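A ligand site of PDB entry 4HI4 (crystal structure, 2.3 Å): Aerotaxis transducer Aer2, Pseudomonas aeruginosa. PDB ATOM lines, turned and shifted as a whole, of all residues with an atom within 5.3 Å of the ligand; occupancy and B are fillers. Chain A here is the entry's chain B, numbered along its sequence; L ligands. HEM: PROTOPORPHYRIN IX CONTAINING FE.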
ATOM      1  N   MET A  19     -25.358  20.457 -10.737  1.00  0.00           N
ATOM      2  CA  MET A  19     -26.070  20.204 -11.973  1.00  0.00           C
ATOM      3  C   MET A  19     -25.055  20.333 -13.121  1.00  0.00           C
ATOM      4  O   MET A  19     -24.171  21.193 -13.076  1.00  0.00           O
ATOM      5  CB  MET A  19     -27.175  21.270 -12.093  1.00  0.00           C
ATOM      6  CG  MET A  19     -27.895  21.378 -13.405  1.00  0.00           C
ATOM      7  SD  MET A  19     -29.073  22.766 -13.299  1.00  0.00           S
ATOM      8  CE  MET A  19     -30.210  22.233 -11.999  1.00  0.00           C
ATOM      9  N   ALA A  21     -24.537  20.684 -17.374  1.00  0.00           N
ATOM     10  CA  ALA A  21     -25.122  20.910 -18.697  1.00  0.00           C
ATOM     11  C   ALA A  21     -24.062  20.645 -19.766  1.00  0.00           C
ATOM     12  O   ALA A  21     -22.860  20.863 -19.549  1.00  0.00           O
ATOM     13  CB  ALA A  21     -25.665  22.333 -18.826  1.00  0.00           C
ATOM     14  N   LEU A  25     -26.254  23.214 -23.779  1.00  0.00           N
ATOM     15  CA  LEU A  25     -26.999  23.756 -22.640  1.00  0.00           C
ATOM     16  C   LEU A  25     -28.183  22.853 -22.274  1.00  0.00           C
ATOM     17  O   LEU A  25     -29.183  23.294 -21.656  1.00  0.00           O
ATOM     18  CB  LEU A  25     -27.447  25.210 -22.887  1.00  0.00           C
ATOM     19  CG  LEU A  25     -26.382  26.289 -23.119  1.00  0.00           C
ATOM     20  CD1 LEU A  25     -26.968  27.677 -22.807  1.00  0.00           C
ATOM     21  CD2 LEU A  25     -25.132  26.031 -22.270  1.00  0.00           C
ATOM     22  N   ILE A  27     -29.388  19.991 -19.789  1.00  0.00           N
ATOM     23  CA  ILE A  27     -29.061  19.410 -18.489  1.00  0.00           C
ATOM     24  C   ILE A  27     -28.886  17.907 -18.654  1.00  0.00           C
ATOM     25  O   ILE A  27     -29.809  17.195 -19.122  1.00  0.00           O
ATOM     26  CB  ILE A  27     -30.191  19.727 -17.466  1.00  0.00           C
ATOM     27  CG1 ILE A  27     -30.327  21.237 -17.289  1.00  0.00           C
ATOM     28  CG2 ILE A  27     -29.927  19.050 -16.126  1.00  0.00           C
ATOM     29  CD1 ILE A  27     -31.424  21.646 -16.314  1.00  0.00           C
ATOM     30  N   ILE A  45     -40.483  28.921  -6.777  1.00  0.00           N
ATOM     31  CA  ILE A  45     -39.981  29.168  -8.123  1.00  0.00           C
ATOM     32  C   ILE A  45     -41.145  29.265  -9.124  1.00  0.00           C
ATOM     33  O   ILE A  45     -41.045  29.960 -10.131  1.00  0.00           O
ATOM     34  CB  ILE A  45     -38.961  28.083  -8.550  1.00  0.00           C
ATOM     35  CG1 ILE A  45     -37.702  28.173  -7.679  1.00  0.00           C
ATOM     36  CG2 ILE A  45     -38.582  28.234 -10.022  1.00  0.00           C
ATOM     37  CD1 ILE A  45     -36.695  27.037  -7.872  1.00  0.00           C
ATOM     38  N   GLN A  48     -42.752  32.747 -10.186  1.00  0.00           N
ATOM     39  CA  GLN A  48     -42.107  33.493 -11.269  1.00  0.00           C
ATOM     40  C   GLN A  48     -42.012  32.655 -12.558  1.00  0.00           C
ATOM     41  O   GLN A  48     -42.014  33.216 -13.656  1.00  0.00           O
ATOM     42  CB  GLN A  48     -40.724  33.937 -10.819  1.00  0.00           C
ATOM     43  CG  GLN A  48     -39.906  34.612 -11.897  1.00  0.00           C
ATOM     44  CD  GLN A  48     -38.611  35.187 -11.361  1.00  0.00           C
ATOM     45  OE1 GLN A  48     -38.522  35.557 -10.181  1.00  0.00           O
ATOM     46  NE2 GLN A  48     -37.604  35.277 -12.225  1.00  0.00           N
ATOM     47  N   LEU A  49     -41.894  31.343 -12.422  1.00  0.00           N
ATOM     48  CA  LEU A  49     -41.889  30.428 -13.565  1.00  0.00           C
ATOM     49  C   LEU A  49     -42.994  29.396 -13.340  1.00  0.00           C
ATOM     50  O   LEU A  49     -42.750  28.317 -12.799  1.00  0.00           O
ATOM     51  CB  LEU A  49     -40.541  29.716 -13.676  1.00  0.00           C
ATOM     52  CG  LEU A  49     -39.332  30.502 -14.178  1.00  0.00           C
ATOM     53  CD1 LEU A  49     -38.053  29.703 -13.989  1.00  0.00           C
ATOM     54  CD2 LEU A  49     -39.504  30.877 -15.632  1.00  0.00           C
ATOM     55  N   PHE A  52     -42.403  25.666 -14.191  1.00  0.00           N
ATOM     56  CA  PHE A  52     -41.222  24.992 -13.656  1.00  0.00           C
ATOM     57  C   PHE A  52     -41.625  23.688 -12.979  1.00  0.00           C
ATOM     58  O   PHE A  52     -42.483  23.674 -12.094  1.00  0.00           O
ATOM     59  CB  PHE A  52     -40.508  25.906 -12.648  1.00  0.00           C
ATOM     60  CG  PHE A  52     -39.334  25.260 -11.958  1.00  0.00           C
ATOM     61  CD1 PHE A  52     -38.099  25.182 -12.588  1.00  0.00           C
ATOM     62  CD2 PHE A  52     -39.459  24.740 -10.672  1.00  0.00           C
ATOM     63  CE1 PHE A  52     -37.006  24.607 -11.942  1.00  0.00           C
ATOM     64  CE2 PHE A  52     -38.374  24.161 -10.030  1.00  0.00           C
ATOM     65  CZ  PHE A  52     -37.146  24.086 -10.672  1.00  0.00           C
ATOM     66  N   LEU A  57     -36.556  18.349 -15.025  1.00  0.00           N
ATOM     67  CA  LEU A  57     -35.338  19.083 -15.385  1.00  0.00           C
ATOM     68  C   LEU A  57     -34.303  18.280 -16.217  1.00  0.00           C
ATOM     69  O   LEU A  57     -33.668  18.813 -17.125  1.00  0.00           O
ATOM     70  CB  LEU A  57     -34.678  19.639 -14.135  1.00  0.00           C
ATOM     71  CG  LEU A  57     -35.371  20.832 -13.476  1.00  0.00           C
ATOM     72  CD1 LEU A  57     -34.587  21.269 -12.230  1.00  0.00           C
ATOM     73  CD2 LEU A  57     -35.540  21.999 -14.473  1.00  0.00           C
ATOM     74  N   ILE A  62     -31.882  24.779 -20.918  1.00  0.00           N
ATOM     75  CA  ILE A  62     -31.992  25.914 -19.985  1.00  0.00           C
ATOM     76  C   ILE A  62     -32.461  27.214 -20.648  1.00  0.00           C
ATOM     77  O   ILE A  62     -32.940  28.133 -19.967  1.00  0.00           O
ATOM     78  CB  ILE A  62     -30.689  26.131 -19.238  1.00  0.00           C
ATOM     79  CG1 ILE A  62     -29.565  26.503 -20.214  1.00  0.00           C
ATOM     80  CG2 ILE A  62     -30.321  24.874 -18.461  1.00  0.00           C
ATOM     81  CD1 ILE A  62     -28.287  26.912 -19.531  1.00  0.00           C
ATOM     82  N   PHE A  65     -35.647  28.785 -19.456  1.00  0.00           N
ATOM     83  CA  PHE A  65     -35.736  29.529 -18.193  1.00  0.00           C
ATOM     84  C   PHE A  65     -35.073  30.915 -18.298  1.00  0.00           C
ATOM     85  O   PHE A  65     -34.999  31.637 -17.309  1.00  0.00           O
ATOM     86  CB  PHE A  65     -35.083  28.755 -17.038  1.00  0.00           C
ATOM     87  CG  PHE A  65     -35.529  27.326 -16.899  1.00  0.00           C
ATOM     88  CD1 PHE A  65     -36.826  27.003 -16.516  1.00  0.00           C
ATOM     89  CD2 PHE A  65     -34.625  26.288 -17.115  1.00  0.00           C
ATOM     90  CE1 PHE A  65     -37.217  25.684 -16.366  1.00  0.00           C
ATOM     91  CE2 PHE A  65     -35.018  24.959 -16.974  1.00  0.00           C
ATOM     92  CZ  PHE A  65     -36.310  24.659 -16.598  1.00  0.00           C
ATOM     93  N   HIS A  66     -34.590  31.263 -19.481  1.00  0.00           N
ATOM     94  CA  HIS A  66     -33.795  32.482 -19.657  1.00  0.00           C
ATOM     95  C   HIS A  66     -34.530  33.451 -20.603  1.00  0.00           C
ATOM     96  O   HIS A  66     -34.992  33.051 -21.690  1.00  0.00           O
ATOM     97  CB  HIS A  66     -32.401  32.132 -20.206  1.00  0.00           C
ATOM     98  CG  HIS A  66     -31.536  31.346 -19.244  1.00  0.00           C
ATOM     99  ND1 HIS A  66     -30.388  30.680 -19.636  1.00  0.00           N
ATOM    100  CD2 HIS A  66     -31.651  31.141 -17.912  1.00  0.00           C
ATOM    101  CE1 HIS A  66     -29.832  30.106 -18.576  1.00  0.00           C
ATOM    102  NE2 HIS A  66     -30.581  30.365 -17.521  1.00  0.00           N
ATOM    103  N   LYS A  67     -34.661  34.708 -20.179  1.00  0.00           N
ATOM    104  CA  LYS A  67     -35.332  35.758 -20.966  1.00  0.00           C
ATOM    105  C   LYS A  67     -34.693  35.945 -22.343  1.00  0.00           C
ATOM    106  O   LYS A  67     -35.381  36.062 -23.351  1.00  0.00           O
ATOM    107  CB  LYS A  67     -35.303  37.099 -20.220  1.00  0.00           C
ATOM    108  CG  LYS A  67     -36.434  37.295 -19.235  1.00  0.00           C
ATOM    109  CD  LYS A  67     -36.566  38.768 -18.823  1.00  0.00           C
ATOM    110  CE  LYS A  67     -37.773  38.994 -17.903  1.00  0.00           C
ATOM    111  NZ  LYS A  67     -38.155  40.433 -17.796  1.00  0.00           N
ATOM    112  N   ASN A  68     -33.370  36.046 -22.356  1.00  0.00           N
ATOM    113  CA  ASN A  68     -32.596  36.186 -23.583  1.00  0.00           C
ATOM    114  C   ASN A  68     -31.665  35.000 -23.750  1.00  0.00           C
ATOM    115  O   ASN A  68     -30.498  35.052 -23.350  1.00  0.00           O
ATOM    116  CB  ASN A  68     -31.805  37.500 -23.572  1.00  0.00           C
ATOM    117  CG  ASN A  68     -32.704  38.706 -23.436  1.00  0.00           C
ATOM    118  OD1 ASN A  68     -33.818  38.736 -24.010  1.00  0.00           O
ATOM    119  ND2 ASN A  68     -32.259  39.710 -22.681  1.00  0.00           N
ATOM    120  N   HIS A  71     -28.012  35.371 -24.731  1.00  0.00           N
ATOM    121  CA  HIS A  71     -27.074  35.946 -23.782  1.00  0.00           C
ATOM    122  C   HIS A  71     -26.287  34.873 -23.038  1.00  0.00           C
ATOM    123  O   HIS A  71     -25.058  34.809 -23.153  1.00  0.00           O
ATOM    124  CB  HIS A  71     -27.789  36.871 -22.786  1.00  0.00           C
ATOM    125  CG  HIS A  71     -26.883  37.514 -21.783  1.00  0.00           C
ATOM    126  ND1 HIS A  71     -25.878  38.391 -22.130  1.00  0.00           N
ATOM    127  CD2 HIS A  71     -26.836  37.405 -20.424  1.00  0.00           C
ATOM    128  CE1 HIS A  71     -25.241  38.790 -21.032  1.00  0.00           C
ATOM    129  NE2 HIS A  71     -25.801  38.200 -19.988  1.00  0.00           N
ATOM    130  N   GLN A  72     -26.999  34.013 -22.315  1.00  0.00           N
ATOM    131  CA  GLN A  72     -26.363  32.917 -21.586  1.00  0.00           C
ATOM    132  C   GLN A  72     -25.542  32.023 -22.487  1.00  0.00           C
ATOM    133  O   GLN A  72     -24.498  31.537 -22.076  1.00  0.00           O
ATOM    134  CB  GLN A  72     -27.379  32.081 -20.807  1.00  0.00           C
ATOM    135  CG  GLN A  72     -27.803  32.682 -19.476  1.00  0.00           C
ATOM    136  CD  GLN A  72     -28.908  33.694 -19.643  1.00  0.00           C
ATOM    137  OE1 GLN A  72     -29.269  34.025 -20.764  1.00  0.00           O
ATOM    138  NE2 GLN A  72     -29.467  34.164 -18.525  1.00  0.00           N
ATOM    139  N   LEU A  75     -22.287  33.886 -23.211  1.00  0.00           N
ATOM    140  CA  LEU A  75     -21.536  33.927 -21.966  1.00  0.00           C
ATOM    141  C   LEU A  75     -20.927  32.559 -21.660  1.00  0.00           C
ATOM    142  O   LEU A  75     -19.713  32.429 -21.502  1.00  0.00           O
ATOM    143  CB  LEU A  75     -22.449  34.373 -20.840  1.00  0.00           C
ATOM    144  CG  LEU A  75     -21.835  34.708 -19.481  1.00  0.00           C
ATOM    145  CD1 LEU A  75     -22.740  35.647 -18.713  1.00  0.00           C
ATOM    146  CD2 LEU A  75     -21.580  33.429 -18.700  1.00  0.00           C
ATOM    147  N   LEU A  76     -21.763  31.533 -21.589  1.00  0.00           N
ATOM    148  CA  LEU A  76     -21.312  30.173 -21.286  1.00  0.00           C
ATOM    149  C   LEU A  76     -20.320  29.599 -22.271  1.00  0.00           C
ATOM    150  O   LEU A  76     -19.383  28.908 -21.880  1.00  0.00           O
ATOM    151  CB  LEU A  76     -22.492  29.212 -21.116  1.00  0.00           C
ATOM    152  CG  LEU A  76     -23.281  29.500 -19.842  1.00  0.00           C
ATOM    153  CD1 LEU A  76     -24.674  28.896 -19.927  1.00  0.00           C
ATOM    154  CD2 LEU A  76     -22.518  28.967 -18.611  1.00  0.00           C
ATOM    155  N   HIS A  83     -17.905  31.445 -13.238  1.00  0.00           N
ATOM    156  CA  HIS A  83     -18.801  32.588 -13.314  1.00  0.00           C
ATOM    157  C   HIS A  83     -19.756  32.525 -12.128  1.00  0.00           C
ATOM    158  O   HIS A  83     -20.399  31.509 -11.900  1.00  0.00           O
ATOM    159  CB  HIS A  83     -19.566  32.602 -14.647  1.00  0.00           C
ATOM    160  CG  HIS A  83     -20.552  33.713 -14.778  1.00  0.00           C
ATOM    161  ND1 HIS A  83     -20.196  34.979 -15.216  1.00  0.00           N
ATOM    162  CD2 HIS A  83     -21.872  33.780 -14.487  1.00  0.00           C
ATOM    163  CE1 HIS A  83     -21.266  35.756 -15.208  1.00  0.00           C
ATOM    164  NE2 HIS A  83     -22.292  35.054 -14.780  1.00  0.00           N
ATOM    165  N   LYS A  84     -19.816  33.599 -11.359  1.00  0.00           N
ATOM    166  CA  LYS A  84     -20.669  33.660 -10.171  1.00  0.00           C
ATOM    167  C   LYS A  84     -21.906  34.525 -10.403  1.00  0.00           C
ATOM    168  O   LYS A  84     -21.829  35.740 -10.396  1.00  0.00           O
ATOM    169  CB  LYS A  84     -19.856  34.137  -8.966  1.00  0.00           C
ATOM    170  CG  LYS A  84     -18.677  33.215  -8.619  1.00  0.00           C
ATOM    171  CD  LYS A  84     -17.849  33.764  -7.456  1.00  0.00           C
ATOM    172  CE  LYS A  84     -18.492  33.473  -6.102  1.00  0.00           C
ATOM    173  NZ  LYS A  84     -18.550  32.019  -5.807  1.00  0.00           N
ATOM    174  N   ALA A  85     -23.033  33.877 -10.620  1.00  0.00           N
ATOM    175  CA  ALA A  85     -24.293  34.578 -10.837  1.00  0.00           C
ATOM    176  C   ALA A  85     -25.182  34.470  -9.600  1.00  0.00           C
ATOM    177  O   ALA A  85     -25.102  33.508  -8.836  1.00  0.00           O
ATOM    178  CB  ALA A  85     -25.020  34.005 -12.059  1.00  0.00           C
ATOM    179  N   LEU A  87     -29.295  34.621  -8.463  1.00  0.00           N
ATOM    180  CA  LEU A  87     -30.683  34.606  -8.956  1.00  0.00           C
ATOM    181  C   LEU A  87     -31.699  34.893  -7.849  1.00  0.00           C
ATOM    182  O   LEU A  87     -31.493  34.538  -6.665  1.00  0.00           O
ATOM    183  CB  LEU A  87     -31.022  33.257  -9.608  1.00  0.00           C
ATOM    184  CG  LEU A  87     -30.165  32.762 -10.770  1.00  0.00           C
ATOM    185  CD1 LEU A  87     -30.800  31.540 -11.396  1.00  0.00           C
ATOM    186  CD2 LEU A  87     -29.968  33.854 -11.807  1.00  0.00           C
ATOM    187  N   LEU A  89     -35.598  33.909  -7.471  1.00  0.00           N
ATOM    188  CA  LEU A  89     -36.726  33.187  -8.070  1.00  0.00           C
ATOM    189  C   LEU A  89     -37.885  33.075  -7.101  1.00  0.00           C
ATOM    190  O   LEU A  89     -37.794  32.333  -6.120  1.00  0.00           O
ATOM    191  CB  LEU A  89     -36.304  31.780  -8.514  1.00  0.00           C
ATOM    192  CG  LEU A  89     -35.270  31.669  -9.640  1.00  0.00           C
ATOM    193  CD1 LEU A  89     -35.211  30.209 -10.130  1.00  0.00           C
ATOM    194  CD2 LEU A  89     -35.608  32.605 -10.769  1.00  0.00           C
ATOM    195  N   LEU A  96     -25.210  30.850  -8.072  1.00  0.00           N
ATOM    196  CA  LEU A  96     -24.720  29.844  -8.984  1.00  0.00           C
ATOM    197  C   LEU A  96     -23.211  30.000  -9.149  1.00  0.00           C
ATOM    198  O   LEU A  96     -22.737  31.082  -9.450  1.00  0.00           O
ATOM    199  CB  LEU A  96     -25.399  29.955 -10.355  1.00  0.00           C
ATOM    200  CG  LEU A  96     -26.698  29.174 -10.618  1.00  0.00           C
ATOM    201  CD1 LEU A  96     -27.649  29.253  -9.441  1.00  0.00           C
ATOM    202  CD2 LEU A  96     -27.384  29.640 -11.895  1.00  0.00           C
ATOM    203  N   VAL A  98     -20.775  28.686 -11.767  1.00  0.00           N
ATOM    204  CA  VAL A  98     -20.683  27.992 -13.054  1.00  0.00           C
ATOM    205  C   VAL A  98     -19.227  27.711 -13.429  1.00  0.00           C
ATOM    206  O   VAL A  98     -18.446  28.640 -13.710  1.00  0.00           O
ATOM    207  CB  VAL A  98     -21.329  28.823 -14.198  1.00  0.00           C
ATOM    208  CG1 VAL A  98     -21.217  28.104 -15.529  1.00  0.00           C
ATOM    209  CG2 VAL A  98     -22.744  29.164 -13.859  1.00  0.00           C
ATOM    210  N   SER A 111     -20.737  22.317 -18.734  1.00  0.00           N
ATOM    211  CA  SER A 111     -20.716  23.180 -17.552  1.00  0.00           C
ATOM    212  C   SER A 111     -21.237  22.439 -16.341  1.00  0.00           C
ATOM    213  O   SER A 111     -22.331  21.803 -16.396  1.00  0.00           O
ATOM    214  CB  SER A 111     -21.556  24.437 -17.761  1.00  0.00           C
ATOM    215  OG  SER A 111     -21.093  25.159 -18.890  1.00  0.00           O
ATOM    216  N   VAL A 113     -22.545  23.254 -12.620  1.00  0.00           N
ATOM    217  CA  VAL A 113     -23.009  24.406 -11.857  1.00  0.00           C
ATOM    218  C   VAL A 113     -23.313  24.018 -10.404  1.00  0.00           C
ATOM    219  O   VAL A 113     -24.101  23.094 -10.159  1.00  0.00           O
ATOM    220  CB  VAL A 113     -24.274  24.992 -12.506  1.00  0.00           C
ATOM    221  CG1 VAL A 113     -24.670  26.303 -11.822  1.00  0.00           C
ATOM    222  CG2 VAL A 113     -24.061  25.193 -14.026  1.00  0.00           C
ATOM    223  N   TRP A 115     -25.246  24.996  -7.125  1.00  0.00           N
ATOM    224  CA  TRP A 115     -26.339  25.819  -6.644  1.00  0.00           C
ATOM    225  C   TRP A 115     -26.276  25.904  -5.128  1.00  0.00           C
ATOM    226  O   TRP A 115     -26.092  24.899  -4.414  1.00  0.00           O
ATOM    227  CB  TRP A 115     -27.696  25.217  -7.013  1.00  0.00           C
ATOM    228  CG  TRP A 115     -28.096  25.293  -8.452  1.00  0.00           C
ATOM    229  CD1 TRP A 115     -27.503  24.641  -9.509  1.00  0.00           C
ATOM    230  CD2 TRP A 115     -29.203  26.010  -9.005  1.00  0.00           C
ATOM    231  NE1 TRP A 115     -28.175  24.924 -10.664  1.00  0.00           N
ATOM    232  CE2 TRP A 115     -29.207  25.772 -10.390  1.00  0.00           C
ATOM    233  CE3 TRP A 115     -30.179  26.853  -8.462  1.00  0.00           C
ATOM    234  CZ2 TRP A 115     -30.163  26.330 -11.244  1.00  0.00           C
ATOM    235  CZ3 TRP A 115     -31.126  27.414  -9.312  1.00  0.00           C
ATOM    236  CH2 TRP A 115     -31.099  27.156 -10.696  1.00  0.00           C
HETATM  237  CHA HEM L   1     -29.595  33.351 -15.607  1.00  0.00           C
HETATM  238  CHB HEM L   1     -33.220  30.309 -14.278  1.00  0.00           C
HETATM  239  CHC HEM L   1     -30.121  26.464 -15.022  1.00  0.00           C
HETATM  240  CHD HEM L   1     -26.563  29.625 -16.365  1.00  0.00           C
HETATM  241  C1A HEM L   1     -30.839  32.773 -15.184  1.00  0.00           C
HETATM  242  C2A HEM L   1     -31.920  33.594 -14.887  1.00  0.00           C
HETATM  243  C3A HEM L   1     -32.953  32.780 -14.516  1.00  0.00           C
HETATM  244  C4A HEM L   1     -32.494  31.414 -14.576  1.00  0.00           C
HETATM  245  CMA HEM L   1     -34.337  33.237 -14.100  1.00  0.00           C
HETATM  246  CAA HEM L   1     -31.879  35.122 -15.001  1.00  0.00           C
HETATM  247  CBA HEM L   1     -32.088  35.523 -16.451  1.00  0.00           C
HETATM  248  CGA HEM L   1     -33.528  35.849 -16.659  1.00  0.00           C
HETATM  249  O1A HEM L   1     -34.250  36.286 -15.712  1.00  0.00           O
HETATM  250  O2A HEM L   1     -34.002  35.671 -17.836  1.00  0.00           O
HETATM  251  C1B HEM L   1     -32.734  28.996 -14.340  1.00  0.00           C
HETATM  252  C2B HEM L   1     -33.465  27.838 -14.036  1.00  0.00           C
HETATM  253  C3B HEM L   1     -32.566  26.713 -14.262  1.00  0.00           C
HETATM  254  C4B HEM L   1     -31.283  27.241 -14.696  1.00  0.00           C
HETATM  255  CMB HEM L   1     -34.832  27.762 -13.583  1.00  0.00           C
HETATM  256  CAB HEM L   1     -32.889  25.361 -14.052  1.00  0.00           C
HETATM  257  CBB HEM L   1     -32.332  24.399 -14.850  1.00  0.00           C
HETATM  258  C1C HEM L   1     -28.875  26.895 -15.466  1.00  0.00           C
HETATM  259  C2C HEM L   1     -27.671  26.175 -15.804  1.00  0.00           C
HETATM  260  C3C HEM L   1     -26.705  27.141 -16.172  1.00  0.00           C
HETATM  261  C4C HEM L   1     -27.274  28.397 -16.065  1.00  0.00           C
HETATM  262  CMC HEM L   1     -27.490  24.811 -15.769  1.00  0.00           C
HETATM  263  CAC HEM L   1     -25.340  26.983 -16.614  1.00  0.00           C
HETATM  264  CBC HEM L   1     -25.035  25.920 -17.470  1.00  0.00           C
HETATM  265  C1D HEM L   1     -27.052  30.955 -16.288  1.00  0.00           C
HETATM  266  C2D HEM L   1     -26.305  32.123 -16.608  1.00  0.00           C
HETATM  267  C3D HEM L   1     -27.182  33.221 -16.402  1.00  0.00           C
HETATM  268  C4D HEM L   1     -28.413  32.661 -15.949  1.00  0.00           C
HETATM  269  CMD HEM L   1     -24.966  32.139 -17.050  1.00  0.00           C
HETATM  270  CAD HEM L   1     -26.899  34.608 -16.563  1.00  0.00           C
HETATM  271  CBD HEM L   1     -25.887  34.910 -15.506  1.00  0.00           C
HETATM  272  CGD HEM L   1     -25.461  36.347 -15.496  1.00  0.00           C
HETATM  273  O1D HEM L   1     -24.809  36.769 -14.494  1.00  0.00           O
HETATM  274  O2D HEM L   1     -25.761  37.096 -16.474  1.00  0.00           O
HETATM  275  NA  HEM L   1     -31.224  31.436 -14.982  1.00  0.00           N
HETATM  276  NB  HEM L   1     -31.547  28.588 -14.837  1.00  0.00           N
HETATM  277  NC  HEM L   1     -28.564  28.158 -15.648  1.00  0.00           N
HETATM  278  ND  HEM L   1     -28.290  31.362 -16.066  1.00  0.00           N
HETATM  279 FE   HEM L   1     -29.729  29.987 -15.281  1.00  0.00          FE
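The backbone carbonyl oxygen (O) of Asn 68 sits close to the side-chain amide oxygen (OE1) of Gln 72. The backbone carbonyl oxygen (O) of Ala 85 is in hydrogen-bond range of the backbone NH (N) of Leu 96, at 2.8 Å. N of Ile 62 is in hydrogen-bond range of O of Leu 25 (3.2 Å). The backbone carbonyl oxygen (O) of Met 19 lies within hydrogen-bond range of the backbone NH (N) of Val 113 (2.7 Å). SD of Met 19 lies within hydrogen-bond range of NE1 of Trp 115, 3.5 Å away. The backbone carbonyl oxygen of Ser 111 sits at hydrogen-bond distance from the backbone NH of Ala 21, 2.7 Å away. O of His 83 sits at hydrogen-bond distance from N of Val 98, at 2.9 Å.
SD of Met 19 touches CMC of the ligand, 3.6 Å away. Ala 21 touches the ligand. CD1 of Ile 27 touches CBB of the ligand, 3.2 Å away. CD1 of Leu 49 touches CMB of the ligand, at 3.8 Å. CD1 of Ile 62 touches C3C of the ligand (3.7 Å). Phe 65 touches the ligand (CG to CMB, 3.4 Å). His 71 touches the ligand. NE2 of Gln 72 touches CHA of the ligand (3.0 Å). Leu 75 touches the ligand (CD2 to CMD, 3.98 Å). Leu 76 touches the ligand (CD1 to CBC, 3.9 Å). Ala 85 touches the ligand (CB to CBD, 3.7 Å). Leu 87 touches the ligand. Leu 89 touches the ligand. Ser 111 touches the ligand (CB to CBC, 3.8 Å). CG2 of Val 113 touches CAC of the ligand (3.4 Å). Trp 115 touches the ligand (CZ2 to C4B, 3.7 Å). Hydrophobic or aromatic side chains that line the ligand: Met 19, Ala 21, Ile 27, Leu 49, Ile 62, Phe 65, His 66, Leu 75, Leu 76, His 83, Ala 85, Leu 87, Leu 89, Val 113 and Trp 115. Of the 28 residues printed, 19 come within 4 Å of the ligand.
A ring nitrogen (NE2) of His 83 sits at hydrogen-bond distance from an oxygen (O1D) of the ligand (3.1 Å). The backbone NH (N) of Lys 67 sits at hydrogen-bond distance from an oxygen (O2A) of the ligand. An iron atom (FE) of the ligand is bound by a ring nitrogen (NE2) of His 66, at 2.4 Å.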
